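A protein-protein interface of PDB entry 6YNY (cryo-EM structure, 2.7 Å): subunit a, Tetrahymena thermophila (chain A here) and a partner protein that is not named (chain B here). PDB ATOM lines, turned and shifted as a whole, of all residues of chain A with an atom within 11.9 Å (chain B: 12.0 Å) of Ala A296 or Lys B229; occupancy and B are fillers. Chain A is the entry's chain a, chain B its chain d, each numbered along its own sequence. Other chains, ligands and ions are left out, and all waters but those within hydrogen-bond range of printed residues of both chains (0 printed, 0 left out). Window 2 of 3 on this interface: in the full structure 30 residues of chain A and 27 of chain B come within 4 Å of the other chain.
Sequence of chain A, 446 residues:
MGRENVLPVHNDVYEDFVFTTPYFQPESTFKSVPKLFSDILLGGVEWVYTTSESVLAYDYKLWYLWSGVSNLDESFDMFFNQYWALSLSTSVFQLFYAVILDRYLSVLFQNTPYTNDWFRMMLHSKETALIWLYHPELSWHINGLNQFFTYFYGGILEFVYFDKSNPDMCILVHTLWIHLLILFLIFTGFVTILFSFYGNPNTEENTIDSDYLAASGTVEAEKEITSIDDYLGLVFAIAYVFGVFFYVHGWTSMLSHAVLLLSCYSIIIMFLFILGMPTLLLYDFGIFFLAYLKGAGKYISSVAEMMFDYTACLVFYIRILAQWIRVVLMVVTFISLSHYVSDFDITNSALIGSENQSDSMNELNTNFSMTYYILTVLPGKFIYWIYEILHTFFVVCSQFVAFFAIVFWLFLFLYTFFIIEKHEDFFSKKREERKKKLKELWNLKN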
ATOM      1  N   ILE A 287     -11.678 -26.042  -5.304  1.00  0.00           N
ATOM      2  CA  ILE A 287     -12.916 -26.705  -4.927  1.00  0.00           C
ATOM      3  C   ILE A 287     -13.632 -25.969  -3.803  1.00  0.00           C
ATOM      4  O   ILE A 287     -14.837 -26.163  -3.607  1.00  0.00           O
ATOM      5  CB  ILE A 287     -12.622 -28.165  -4.542  1.00  0.00           C
ATOM      6  CG1 ILE A 287     -13.913 -28.975  -4.484  1.00  0.00           C
ATOM      7  CG2 ILE A 287     -11.906 -28.232  -3.217  1.00  0.00           C
ATOM      8  CD1 ILE A 287     -14.589 -29.126  -5.815  1.00  0.00           C
ATOM      9  N   PHE A 288     -12.923 -25.128  -3.055  1.00  0.00           N
ATOM     10  CA  PHE A 288     -13.517 -24.307  -2.011  1.00  0.00           C
ATOM     11  C   PHE A 288     -14.143 -23.027  -2.541  1.00  0.00           C
ATOM     12  O   PHE A 288     -14.515 -22.165  -1.741  1.00  0.00           O
ATOM     13  CB  PHE A 288     -12.460 -23.939  -0.968  1.00  0.00           C
ATOM     14  CG  PHE A 288     -11.997 -25.090  -0.135  1.00  0.00           C
ATOM     15  CD1 PHE A 288     -12.330 -25.164   1.203  1.00  0.00           C
ATOM     16  CD2 PHE A 288     -11.224 -26.092  -0.682  1.00  0.00           C
ATOM     17  CE1 PHE A 288     -11.902 -26.216   1.973  1.00  0.00           C
ATOM     18  CE2 PHE A 288     -10.795 -27.145   0.086  1.00  0.00           C
ATOM     19  CZ  PHE A 288     -11.136 -27.209   1.412  1.00  0.00           C
ATOM     20  N   PHE A 289     -14.279 -22.890  -3.861  1.00  0.00           N
ATOM     21  CA  PHE A 289     -14.688 -21.614  -4.437  1.00  0.00           C
ATOM     22  C   PHE A 289     -15.996 -21.108  -3.850  1.00  0.00           C
ATOM     23  O   PHE A 289     -16.223 -19.895  -3.804  1.00  0.00           O
ATOM     24  CB  PHE A 289     -14.796 -21.745  -5.953  1.00  0.00           C
ATOM     25  CG  PHE A 289     -15.900 -22.647  -6.413  1.00  0.00           C
ATOM     26  CD1 PHE A 289     -15.766 -24.017  -6.338  1.00  0.00           C
ATOM     27  CD2 PHE A 289     -17.062 -22.125  -6.945  1.00  0.00           C
ATOM     28  CE1 PHE A 289     -16.772 -24.847  -6.766  1.00  0.00           C
ATOM     29  CE2 PHE A 289     -18.070 -22.953  -7.374  1.00  0.00           C
ATOM     30  CZ  PHE A 289     -17.924 -24.315  -7.284  1.00  0.00           C
ATOM     31  N   LEU A 290     -16.860 -22.007  -3.384  1.00  0.00           N
ATOM     32  CA  LEU A 290     -18.145 -21.574  -2.852  1.00  0.00           C
ATOM     33  C   LEU A 290     -17.999 -20.898  -1.497  1.00  0.00           C
ATOM     34  O   LEU A 290     -18.781 -20.000  -1.168  1.00  0.00           O
ATOM     35  CB  LEU A 290     -19.091 -22.763  -2.755  1.00  0.00           C
ATOM     36  CG  LEU A 290     -19.579 -23.304  -4.093  1.00  0.00           C
ATOM     37  CD1 LEU A 290     -20.344 -24.584  -3.894  1.00  0.00           C
ATOM     38  CD2 LEU A 290     -20.438 -22.277  -4.796  1.00  0.00           C
ATOM     39  N   ALA A 291     -17.015 -21.310  -0.701  1.00  0.00           N
ATOM     40  CA  ALA A 291     -16.762 -20.631   0.563  1.00  0.00           C
ATOM     41  C   ALA A 291     -16.175 -19.245   0.348  1.00  0.00           C
ATOM     42  O   ALA A 291     -16.383 -18.351   1.175  1.00  0.00           O
ATOM     43  CB  ALA A 291     -15.829 -21.472   1.427  1.00  0.00           C
ATOM     44  N   TYR A 292     -15.444 -19.047  -0.748  1.00  0.00           N
ATOM     45  CA  TYR A 292     -14.916 -17.724  -1.051  1.00  0.00           C
ATOM     46  C   TYR A 292     -16.030 -16.738  -1.369  1.00  0.00           C
ATOM     47  O   TYR A 292     -15.859 -15.529  -1.182  1.00  0.00           O
ATOM     48  CB  TYR A 292     -13.940 -17.807  -2.222  1.00  0.00           C
ATOM     49  CG  TYR A 292     -12.633 -18.494  -1.911  1.00  0.00           C
ATOM     50  CD1 TYR A 292     -12.543 -19.873  -1.867  1.00  0.00           C
ATOM     51  CD2 TYR A 292     -11.485 -17.761  -1.677  1.00  0.00           C
ATOM     52  CE1 TYR A 292     -11.352 -20.499  -1.587  1.00  0.00           C
ATOM     53  CE2 TYR A 292     -10.291 -18.379  -1.399  1.00  0.00           C
ATOM     54  CZ  TYR A 292     -10.227 -19.746  -1.355  1.00  0.00           C
ATOM     55  OH  TYR A 292      -9.030 -20.360  -1.076  1.00  0.00           O
ATOM     56  N   LEU A 293     -17.170 -17.229  -1.851  1.00  0.00           N
ATOM     57  CA  LEU A 293     -18.280 -16.365  -2.237  1.00  0.00           C
ATOM     58  C   LEU A 293     -19.262 -16.152  -1.089  1.00  0.00           C
ATOM     59  O   LEU A 293     -19.483 -15.018  -0.654  1.00  0.00           O
ATOM     60  CB  LEU A 293     -19.015 -16.967  -3.437  1.00  0.00           C
ATOM     61  CG  LEU A 293     -18.168 -17.363  -4.639  1.00  0.00           C
ATOM     62  CD1 LEU A 293     -19.031 -18.062  -5.653  1.00  0.00           C
ATOM     63  CD2 LEU A 293     -17.516 -16.157  -5.250  1.00  0.00           C
ATOM     64  N   LYS A 294     -19.853 -17.236  -0.594  1.00  0.00           N
ATOM     65  CA  LYS A 294     -20.917 -17.151   0.397  1.00  0.00           C
ATOM     66  C   LYS A 294     -20.412 -17.286   1.824  1.00  0.00           C
ATOM     67  O   LYS A 294     -21.030 -16.736   2.743  1.00  0.00           O
ATOM     68  CB  LYS A 294     -21.961 -18.237   0.130  1.00  0.00           C
ATOM     69  CG  LYS A 294     -23.215 -18.111   0.972  1.00  0.00           C
ATOM     70  CD  LYS A 294     -24.168 -19.267   0.737  1.00  0.00           C
ATOM     71  CE  LYS A 294     -23.665 -20.536   1.396  1.00  0.00           C
ATOM     72  NZ  LYS A 294     -24.604 -21.678   1.227  1.00  0.00           N
ATOM     73  N   GLY A 295     -19.314 -18.000   2.031  1.00  0.00           N
ATOM     74  CA  GLY A 295     -18.805 -18.228   3.366  1.00  0.00           C
ATOM     75  C   GLY A 295     -19.203 -19.581   3.909  1.00  0.00           C
ATOM     76  O   GLY A 295     -19.383 -20.536   3.148  1.00  0.00           O
ATOM     77  N   ALA A 296     -19.353 -19.674   5.225  1.00  0.00           N
ATOM     78  CA  ALA A 296     -19.708 -20.931   5.862  1.00  0.00           C
ATOM     79  C   ALA A 296     -21.211 -21.158   5.798  1.00  0.00           C
ATOM     80  O   ALA A 296     -22.004 -20.217   5.888  1.00  0.00           O
ATOM     81  CB  ALA A 296     -19.242 -20.946   7.314  1.00  0.00           C
ATOM     82  N   GLY A 297     -21.596 -22.418   5.640  1.00  0.00           N
ATOM     83  CA  GLY A 297     -22.993 -22.779   5.575  1.00  0.00           C
ATOM     84  C   GLY A 297     -23.689 -22.600   6.908  1.00  0.00           C
ATOM     85  O   GLY A 297     -23.110 -22.179   7.910  1.00  0.00           O
ATOM     86  N   LYS A 298     -24.976 -22.936   6.910  1.00  0.00           N
ATOM     87  CA  LYS A 298     -25.796 -22.799   8.106  1.00  0.00           C
ATOM     88  C   LYS A 298     -26.507 -24.099   8.460  1.00  0.00           C
ATOM     89  O   LYS A 298     -26.686 -24.408   9.641  1.00  0.00           O
ATOM     90  CB  LYS A 298     -26.818 -21.680   7.911  1.00  0.00           C
ATOM     91  CG  LYS A 298     -27.540 -21.285   9.179  1.00  0.00           C
ATOM     92  CD  LYS A 298     -28.497 -20.138   8.934  1.00  0.00           C
ATOM     93  CE  LYS A 298     -29.133 -19.667  10.230  1.00  0.00           C
ATOM     94  NZ  LYS A 298     -29.859 -20.761  10.933  1.00  0.00           N
ATOM     95  N   TYR A 299     -26.907 -24.868   7.453  1.00  0.00           N
ATOM     96  CA  TYR A 299     -27.682 -26.080   7.659  1.00  0.00           C
ATOM     97  C   TYR A 299     -26.856 -27.316   7.330  1.00  0.00           C
ATOM     98  O   TYR A 299     -25.993 -27.294   6.451  1.00  0.00           O
ATOM     99  CB  TYR A 299     -28.942 -26.070   6.794  1.00  0.00           C
ATOM    100  CG  TYR A 299     -29.731 -24.788   6.879  1.00  0.00           C
ATOM    101  CD1 TYR A 299     -29.703 -23.867   5.845  1.00  0.00           C
ATOM    102  CD2 TYR A 299     -30.493 -24.492   7.996  1.00  0.00           C
ATOM    103  CE1 TYR A 299     -30.418 -22.693   5.917  1.00  0.00           C
ATOM    104  CE2 TYR A 299     -31.211 -23.322   8.078  1.00  0.00           C
ATOM    105  CZ  TYR A 299     -31.169 -22.424   7.036  1.00  0.00           C
ATOM    106  OH  TYR A 299     -31.884 -21.255   7.119  1.00  0.00           O
ATOM    107  N   ILE A 300     -27.147 -28.404   8.047  1.00  0.00           N
ATOM    108  CA  ILE A 300     -26.446 -29.662   7.834  1.00  0.00           C
ATOM    109  C   ILE A 300     -26.828 -30.320   6.520  1.00  0.00           C
ATOM    110  O   ILE A 300     -26.131 -31.235   6.066  1.00  0.00           O
ATOM    111  CB  ILE A 300     -26.719 -30.627   9.002  1.00  0.00           C
ATOM    112  CG1 ILE A 300     -28.211 -30.940   9.098  1.00  0.00           C
ATOM    113  CG2 ILE A 300     -26.232 -30.032  10.299  1.00  0.00           C
ATOM    114  CD1 ILE A 300     -28.561 -31.851  10.231  1.00  0.00           C
ATOM    115  N   SER A 301     -27.916 -29.888   5.894  1.00  0.00           N
ATOM    116  CA  SER A 301     -28.377 -30.502   4.658  1.00  0.00           C
ATOM    117  C   SER A 301     -27.542 -30.004   3.488  1.00  0.00           C
ATOM    118  O   SER A 301     -27.493 -28.800   3.219  1.00  0.00           O
ATOM    119  CB  SER A 301     -29.852 -30.194   4.430  1.00  0.00           C
ATOM    120  OG  SER A 301     -30.310 -30.781   3.227  1.00  0.00           O
ATOM    121  N   SER A 302     -26.888 -30.932   2.790  1.00  0.00           N
ATOM    122  CA  SER A 302     -26.120 -30.554   1.612  1.00  0.00           C
ATOM    123  C   SER A 302     -27.030 -30.134   0.469  1.00  0.00           C
ATOM    124  O   SER A 302     -26.651 -29.286  -0.344  1.00  0.00           O
ATOM    125  CB  SER A 302     -25.223 -31.710   1.180  1.00  0.00           C
ATOM    126  OG  SER A 302     -25.987 -32.863   0.889  1.00  0.00           O
ATOM    127  N   ALA A 304     -29.847 -28.520   0.862  1.00  0.00           N
ATOM    128  CA  ALA A 304     -30.274 -27.163   1.173  1.00  0.00           C
ATOM    129  C   ALA A 304     -29.204 -26.157   0.780  1.00  0.00           C
ATOM    130  O   ALA A 304     -29.471 -25.202   0.041  1.00  0.00           O
ATOM    131  CB  ALA A 304     -30.597 -27.043   2.660  1.00  0.00           C
ATOM    132  N   GLU A 305     -27.978 -26.358   1.264  1.00  0.00           N
ATOM    133  CA  GLU A 305     -26.893 -25.459   0.900  1.00  0.00           C
ATOM    134  C   GLU A 305     -26.647 -25.470  -0.600  1.00  0.00           C
ATOM    135  O   GLU A 305     -26.283 -24.439  -1.175  1.00  0.00           O
ATOM    136  CB  GLU A 305     -25.621 -25.848   1.648  1.00  0.00           C
ATOM    137  CG  GLU A 305     -25.752 -25.780   3.156  1.00  0.00           C
ATOM    138  CD  GLU A 305     -26.056 -24.383   3.656  1.00  0.00           C
ATOM    139  OE1 GLU A 305     -25.900 -23.421   2.876  1.00  0.00           O
ATOM    140  OE2 GLU A 305     -26.456 -24.246   4.830  1.00  0.00           O
ATOM    141  N   MET A 306     -26.850 -26.616  -1.250  1.00  0.00           N
ATOM    142  CA  MET A 306     -26.658 -26.690  -2.692  1.00  0.00           C
ATOM    143  C   MET A 306     -27.449 -25.609  -3.410  1.00  0.00           C
ATOM    144  O   MET A 306     -26.994 -25.075  -4.427  1.00  0.00           O
ATOM    145  CB  MET A 306     -27.071 -28.071  -3.202  1.00  0.00           C
ATOM    146  CG  MET A 306     -26.787 -28.301  -4.670  1.00  0.00           C
ATOM    147  SD  MET A 306     -27.597 -29.769  -5.327  1.00  0.00           S
ATOM    148  CE  MET A 306     -26.814 -31.048  -4.354  1.00  0.00           C
ATOM    149  N   MET A 307     -28.631 -25.268  -2.896  1.00  0.00           N
ATOM    150  CA  MET A 307     -29.442 -24.238  -3.529  1.00  0.00           C
ATOM    151  C   MET A 307     -28.912 -22.848  -3.214  1.00  0.00           C
ATOM    152  O   MET A 307     -28.868 -21.982  -4.094  1.00  0.00           O
ATOM    153  CB  MET A 307     -30.895 -24.367  -3.079  1.00  0.00           C
ATOM    154  CG  MET A 307     -31.432 -25.782  -3.135  1.00  0.00           C
ATOM    155  SD  MET A 307     -31.155 -26.599  -4.717  1.00  0.00           S
ATOM    156  CE  MET A 307     -32.120 -25.565  -5.809  1.00  0.00           C
ATOM    157  N   PHE A 308     -28.509 -22.615  -1.964  1.00  0.00           N
ATOM    158  CA  PHE A 308     -27.942 -21.326  -1.599  1.00  0.00           C
ATOM    159  C   PHE A 308     -26.595 -21.091  -2.260  1.00  0.00           C
ATOM    160  O   PHE A 308     -26.197 -19.934  -2.434  1.00  0.00           O
ATOM    161  CB  PHE A 308     -27.808 -21.228  -0.082  1.00  0.00           C
ATOM    162  CG  PHE A 308     -29.118 -21.085   0.630  1.00  0.00           C
ATOM    163  CD1 PHE A 308     -29.544 -19.851   1.082  1.00  0.00           C
ATOM    164  CD2 PHE A 308     -29.930 -22.184   0.835  1.00  0.00           C
ATOM    165  CE1 PHE A 308     -30.753 -19.719   1.731  1.00  0.00           C
ATOM    166  CE2 PHE A 308     -31.137 -22.057   1.483  1.00  0.00           C
ATOM    167  CZ  PHE A 308     -31.549 -20.825   1.931  1.00  0.00           C
ATOM    168  N   ASP A 309     -25.889 -22.157  -2.633  1.00  0.00           N
ATOM    169  CA  ASP A 309     -24.617 -22.003  -3.323  1.00  0.00           C
ATOM    170  C   ASP A 309     -24.812 -21.733  -4.806  1.00  0.00           C
ATOM    171  O   ASP A 309     -23.995 -21.036  -5.416  1.00  0.00           O
ATOM    172  CB  ASP A 309     -23.759 -23.249  -3.116  1.00  0.00           C
ATOM    173  CG  ASP A 309     -23.197 -23.342  -1.711  1.00  0.00           C
ATOM    174  OD1 ASP A 309     -23.948 -23.709  -0.785  1.00  0.00           O
ATOM    175  OD2 ASP A 309     -22.002 -23.041  -1.526  1.00  0.00           O
ATOM    176  N   THR A 311     -27.255 -19.911  -5.963  1.00  0.00           N
ATOM    177  CA  THR A 311     -27.576 -18.490  -6.011  1.00  0.00           C
ATOM    178  C   THR A 311     -26.310 -17.647  -5.958  1.00  0.00           C
ATOM    179  O   THR A 311     -26.130 -16.723  -6.759  1.00  0.00           O
ATOM    180  CB  THR A 311     -28.506 -18.121  -4.857  1.00  0.00           C
ATOM    181  OG1 THR A 311     -27.880 -18.452  -3.614  1.00  0.00           O
ATOM    182  CG2 THR A 311     -29.812 -18.873  -4.970  1.00  0.00           C
ATOM    183  N   ALA A 312     -25.415 -17.959  -5.022  1.00  0.00           N
ATOM    184  CA  ALA A 312     -24.180 -17.196  -4.899  1.00  0.00           C
ATOM    185  C   ALA A 312     -23.357 -17.268  -6.177  1.00  0.00           C
ATOM    186  O   ALA A 312     -22.719 -16.284  -6.569  1.00  0.00           O
ATOM    187  CB  ALA A 312     -23.370 -17.706  -3.710  1.00  0.00           C
ATOM    188  N   LEU A 414     -13.922  -7.187  -3.761  1.00  0.00           N
ATOM    189  CA  LEU A 414     -14.775  -8.025  -2.933  1.00  0.00           C
ATOM    190  C   LEU A 414     -14.280  -9.459  -2.826  1.00  0.00           C
ATOM    191  O   LEU A 414     -14.454 -10.086  -1.775  1.00  0.00           O
ATOM    192  CB  LEU A 414     -16.197  -8.029  -3.494  1.00  0.00           C
ATOM    193  CG  LEU A 414     -16.907  -6.679  -3.549  1.00  0.00           C
ATOM    194  CD1 LEU A 414     -18.215  -6.813  -4.283  1.00  0.00           C
ATOM    195  CD2 LEU A 414     -17.137  -6.127  -2.161  1.00  0.00           C
ATOM    196  N   ALA B 225      -6.375 -14.470  -1.959  1.00  0.00           N
ATOM    197  CA  ALA B 225      -7.792 -14.766  -1.838  1.00  0.00           C
ATOM    198  C   ALA B 225      -7.991 -15.736  -0.690  1.00  0.00           C
ATOM    199  O   ALA B 225      -7.225 -16.690  -0.545  1.00  0.00           O
ATOM    200  CB  ALA B 225      -8.347 -15.357  -3.135  1.00  0.00           C
ATOM    201  N   LYS B 226      -9.018 -15.489   0.118  1.00  0.00           N
ATOM    202  CA  LYS B 226      -9.302 -16.329   1.267  1.00  0.00           C
ATOM    203  C   LYS B 226     -10.802 -16.539   1.391  1.00  0.00           C
ATOM    204  O   LYS B 226     -11.609 -15.781   0.849  1.00  0.00           O
ATOM    205  CB  LYS B 226      -8.751 -15.723   2.561  1.00  0.00           C
ATOM    206  CG  LYS B 226      -9.405 -14.432   2.971  1.00  0.00           C
ATOM    207  CD  LYS B 226      -8.810 -13.914   4.258  1.00  0.00           C
ATOM    208  CE  LYS B 226      -9.447 -12.618   4.675  1.00  0.00           C
ATOM    209  NZ  LYS B 226      -8.874 -12.124   5.940  1.00  0.00           N
ATOM    210  N   ALA B 227     -11.159 -17.596   2.112  1.00  0.00           N
ATOM    211  CA  ALA B 227     -12.540 -17.927   2.418  1.00  0.00           C
ATOM    212  C   ALA B 227     -12.720 -17.944   3.925  1.00  0.00           C
ATOM    213  O   ALA B 227     -11.936 -18.574   4.641  1.00  0.00           O
ATOM    214  CB  ALA B 227     -12.926 -19.277   1.828  1.00  0.00           C
ATOM    215  N   THR B 228     -13.743 -17.249   4.402  1.00  0.00           N
ATOM    216  CA  THR B 228     -14.034 -17.145   5.820  1.00  0.00           C
ATOM    217  C   THR B 228     -15.442 -17.656   6.098  1.00  0.00           C
ATOM    218  O   THR B 228     -16.155 -18.111   5.202  1.00  0.00           O
ATOM    219  CB  THR B 228     -13.888 -15.701   6.301  1.00  0.00           C
ATOM    220  OG1 THR B 228     -14.850 -14.875   5.637  1.00  0.00           O
ATOM    221  CG2 THR B 228     -12.506 -15.181   6.005  1.00  0.00           C
ATOM    222  N   LYS B 229     -15.835 -17.578   7.369  1.00  0.00           N
ATOM    223  CA  LYS B 229     -17.201 -17.919   7.742  1.00  0.00           C
ATOM    224  C   LYS B 229     -18.198 -16.932   7.159  1.00  0.00           C
ATOM    225  O   LYS B 229     -19.347 -17.296   6.891  1.00  0.00           O
ATOM    226  CB  LYS B 229     -17.332 -17.960   9.261  1.00  0.00           C
ATOM    227  CG  LYS B 229     -17.069 -16.634   9.934  1.00  0.00           C
ATOM    228  CD  LYS B 229     -17.162 -16.755  11.431  1.00  0.00           C
ATOM    229  CE  LYS B 229     -17.074 -15.406  12.107  1.00  0.00           C
ATOM    230  NZ  LYS B 229     -18.236 -14.543  11.778  1.00  0.00           N
ATOM    231  N   ASN B 230     -17.778 -15.690   6.958  1.00  0.00           N
ATOM    232  CA  ASN B 230     -18.606 -14.674   6.337  1.00  0.00           C
ATOM    233  C   ASN B 230     -18.352 -14.627   4.835  1.00  0.00           C
ATOM    234  O   ASN B 230     -17.391 -15.202   4.321  1.00  0.00           O
ATOM    235  CB  ASN B 230     -18.324 -13.315   6.968  1.00  0.00           C
ATOM    236  CG  ASN B 230     -18.480 -13.331   8.470  1.00  0.00           C
ATOM    237  OD1 ASN B 230     -19.404 -13.942   9.006  1.00  0.00           O
ATOM    238  ND2 ASN B 230     -17.567 -12.667   9.162  1.00  0.00           N
ATOM    239  N   MET B 231     -19.232 -13.930   4.127  1.00  0.00           N
ATOM    240  CA  MET B 231     -19.112 -13.847   2.683  1.00  0.00           C
ATOM    241  C   MET B 231     -18.089 -12.791   2.284  1.00  0.00           C
ATOM    242  O   MET B 231     -17.713 -11.917   3.069  1.00  0.00           O
ATOM    243  CB  MET B 231     -20.460 -13.526   2.042  1.00  0.00           C
ATOM    244  CG  MET B 231     -21.081 -12.222   2.483  1.00  0.00           C
ATOM    245  SD  MET B 231     -21.917 -11.387   1.122  1.00  0.00           S
ATOM    246  CE  MET B 231     -22.966 -12.702   0.516  1.00  0.00           C
ATOM    247  N   LEU B 232     -17.638 -12.886   1.035  1.00  0.00           N
ATOM    248  CA  LEU B 232     -16.702 -11.925   0.463  1.00  0.00           C
ATOM    249  C   LEU B 232     -15.385 -11.897   1.227  1.00  0.00           C
ATOM    250  O   LEU B 232     -14.678 -10.888   1.230  1.00  0.00           O
ATOM    251  CB  LEU B 232     -17.322 -10.528   0.415  1.00  0.00           C
ATOM    252  CG  LEU B 232     -18.713 -10.481  -0.214  1.00  0.00           C
ATOM    253  CD1 LEU B 232     -19.312  -9.098  -0.101  1.00  0.00           C
ATOM    254  CD2 LEU B 232     -18.659 -10.918  -1.656  1.00  0.00           C
ATOM    255  N   GLY B 233     -15.044 -13.004   1.879  1.00  0.00           N
ATOM    256  CA  GLY B 233     -13.793 -13.080   2.601  1.00  0.00           C
ATOM    257  C   GLY B 233     -13.707 -12.184   3.810  1.00  0.00           C
ATOM    258  O   GLY B 233     -12.606 -11.925   4.300  1.00  0.00           O
ATOM    259  N   ARG B 234     -14.838 -11.701   4.309  1.00  0.00           N
ATOM    260  CA  ARG B 234     -14.851 -10.850   5.488  1.00  0.00           C
ATOM    261  C   ARG B 234     -15.113 -11.668   6.746  1.00  0.00           C
ATOM    262  O   ARG B 234     -14.232 -12.376   7.235  1.00  0.00           O
ATOM    263  CB  ARG B 234     -15.904  -9.754   5.346  1.00  0.00           C
ATOM    264  CG  ARG B 234     -15.405  -8.497   4.662  1.00  0.00           C
ATOM    265  CD  ARG B 234     -15.048  -8.740   3.221  1.00  0.00           C
ATOM    266  NE  ARG B 234     -14.505  -7.545   2.590  1.00  0.00           N
ATOM    267  CZ  ARG B 234     -14.155  -7.471   1.313  1.00  0.00           C
ATOM    268  NH1 ARG B 234     -14.291  -8.522   0.523  1.00  0.00           N
ATOM    269  NH2 ARG B 234     -13.667  -6.344   0.824  1.00  0.00           N
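Of the 10 printed residues of chain B, 9 touch a printed residue of chain A. Printed residues of chain A that touch a printed residue of chain B: Ala A291, Tyr A292, Leu A293, Lys A294, Gly A295, Ala A296 and Leu A414. Hydrophobic or aromatic side chains of chain A that line the printed part of chain B: Ala A291, Tyr A292 and Ala A296. Among the printed residues, no Asp or Glu carboxylate lies within 4 Å of a Lys or Arg side-chain nitrogen of the other chain.
The side-chain amino group (NZ) of Lys B229 sits at hydrogen-bond distance from the side-chain amide oxygen (OD1) of Asn B230 (3.1 Å). The backbone carbonyl oxygen (O) of Leu B232 sits at hydrogen-bond distance from the guanidinium group (NH1) of Arg B234. The backbone carbonyl oxygen (O) of Asn B230 sits at hydrogen-bond distance from the side-chain hydroxyl (OG1) of Thr B228, 2.9 Å away. The side-chain amino group (NZ) of Lys A294 is in salt-bridge range of the side-chain carboxylate (OD1) of Asp A309. The side-chain amino group (NZ) of Lys A294 is in salt-bridge range of the side-chain carboxylate (OE1) of Glu A305, 2.7 Å away. OG1 of Thr B228 sits at hydrogen-bond distance from O of Arg B234, 3.0 Å away.
Ala A296 touches just these residues of chain B: Thr B228 (3.6 Å) and Lys B229 (2.9 Å). Of the printed residues of chain A, Lys B229 touches Gly A295 (3.7 Å) and Ala A296 (2.9 Å). Printed residues of chain B within 4 Å of Ala A291: Ala B227 (3.6 Å). Of the printed residues of chain B, Gly A295 touches Thr B228, Lys B229 and Asn B230. No residue of chain B comes within 4 Å of Gly A297. Of chain A, only Ala A291 and Tyr A292 come within 4 Å of Ala B227. Of the printed residues of chain A, Met B231 touches Leu A293 and Lys A294. Of the printed residues of chain A, Lys B226 touches Tyr A292. Printed residues of chain B within 4 Å of Leu A414: Leu B232 and Arg B234. Of the printed residues of chain A, Ala B225 touches Tyr A292. Printed residues of chain B within 4 Å of Tyr A292: Ala B225, Lys B226, Ala B227 and Leu B232. Phe A289 touches none of the printed residues of chain B. Ala A312 touches none of the printed residues of chain B. The nearest residue of chain A that does not touch Lys B229 is Lys A294 (4.5 Å). The nearest printed residue of chain A that does not touch Leu B232 is Lys A294 (5.1 Å).
The guanidinium group (NH1) of Arg B234 is in hydrogen-bond range of the backbone carbonyl oxygen (O) of Leu A414 (2.8 Å). O of Leu B232 sits close to O of Leu A414 (3.1 Å). The backbone NH of Ala A296 is in hydrogen-bond range of the backbone carbonyl oxygen of Lys B229 (2.9 Å). The backbone carbonyl oxygen (O) of Leu A293 lies within hydrogen-bond range of the backbone NH (N) of Leu B232 (3.3 Å).
Among the printed residues, pairs that only touch across the chains: Ala A291 with Ala B227 (3.6 Å), Tyr A292 with Ala B225 (3.6 Å), Tyr A292 with Lys B226 (3.2 Å), Tyr A292 with Ala B227 (3.6 Å), Tyr A292 with Leu B232 (3.9 Å), Leu A293 with Met B231 (3.2 Å), Lys A294 with Asn B230 (3.9995 Å), Lys A294 with Met B231 (3.3 Å), Gly A295 with Thr B228 (3.2 Å), Gly A295 with Lys B229 (3.7 Å), Gly A295 with Asn B230 (3.5 Å) and Ala A296 with Thr B228 (3.6 Å).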
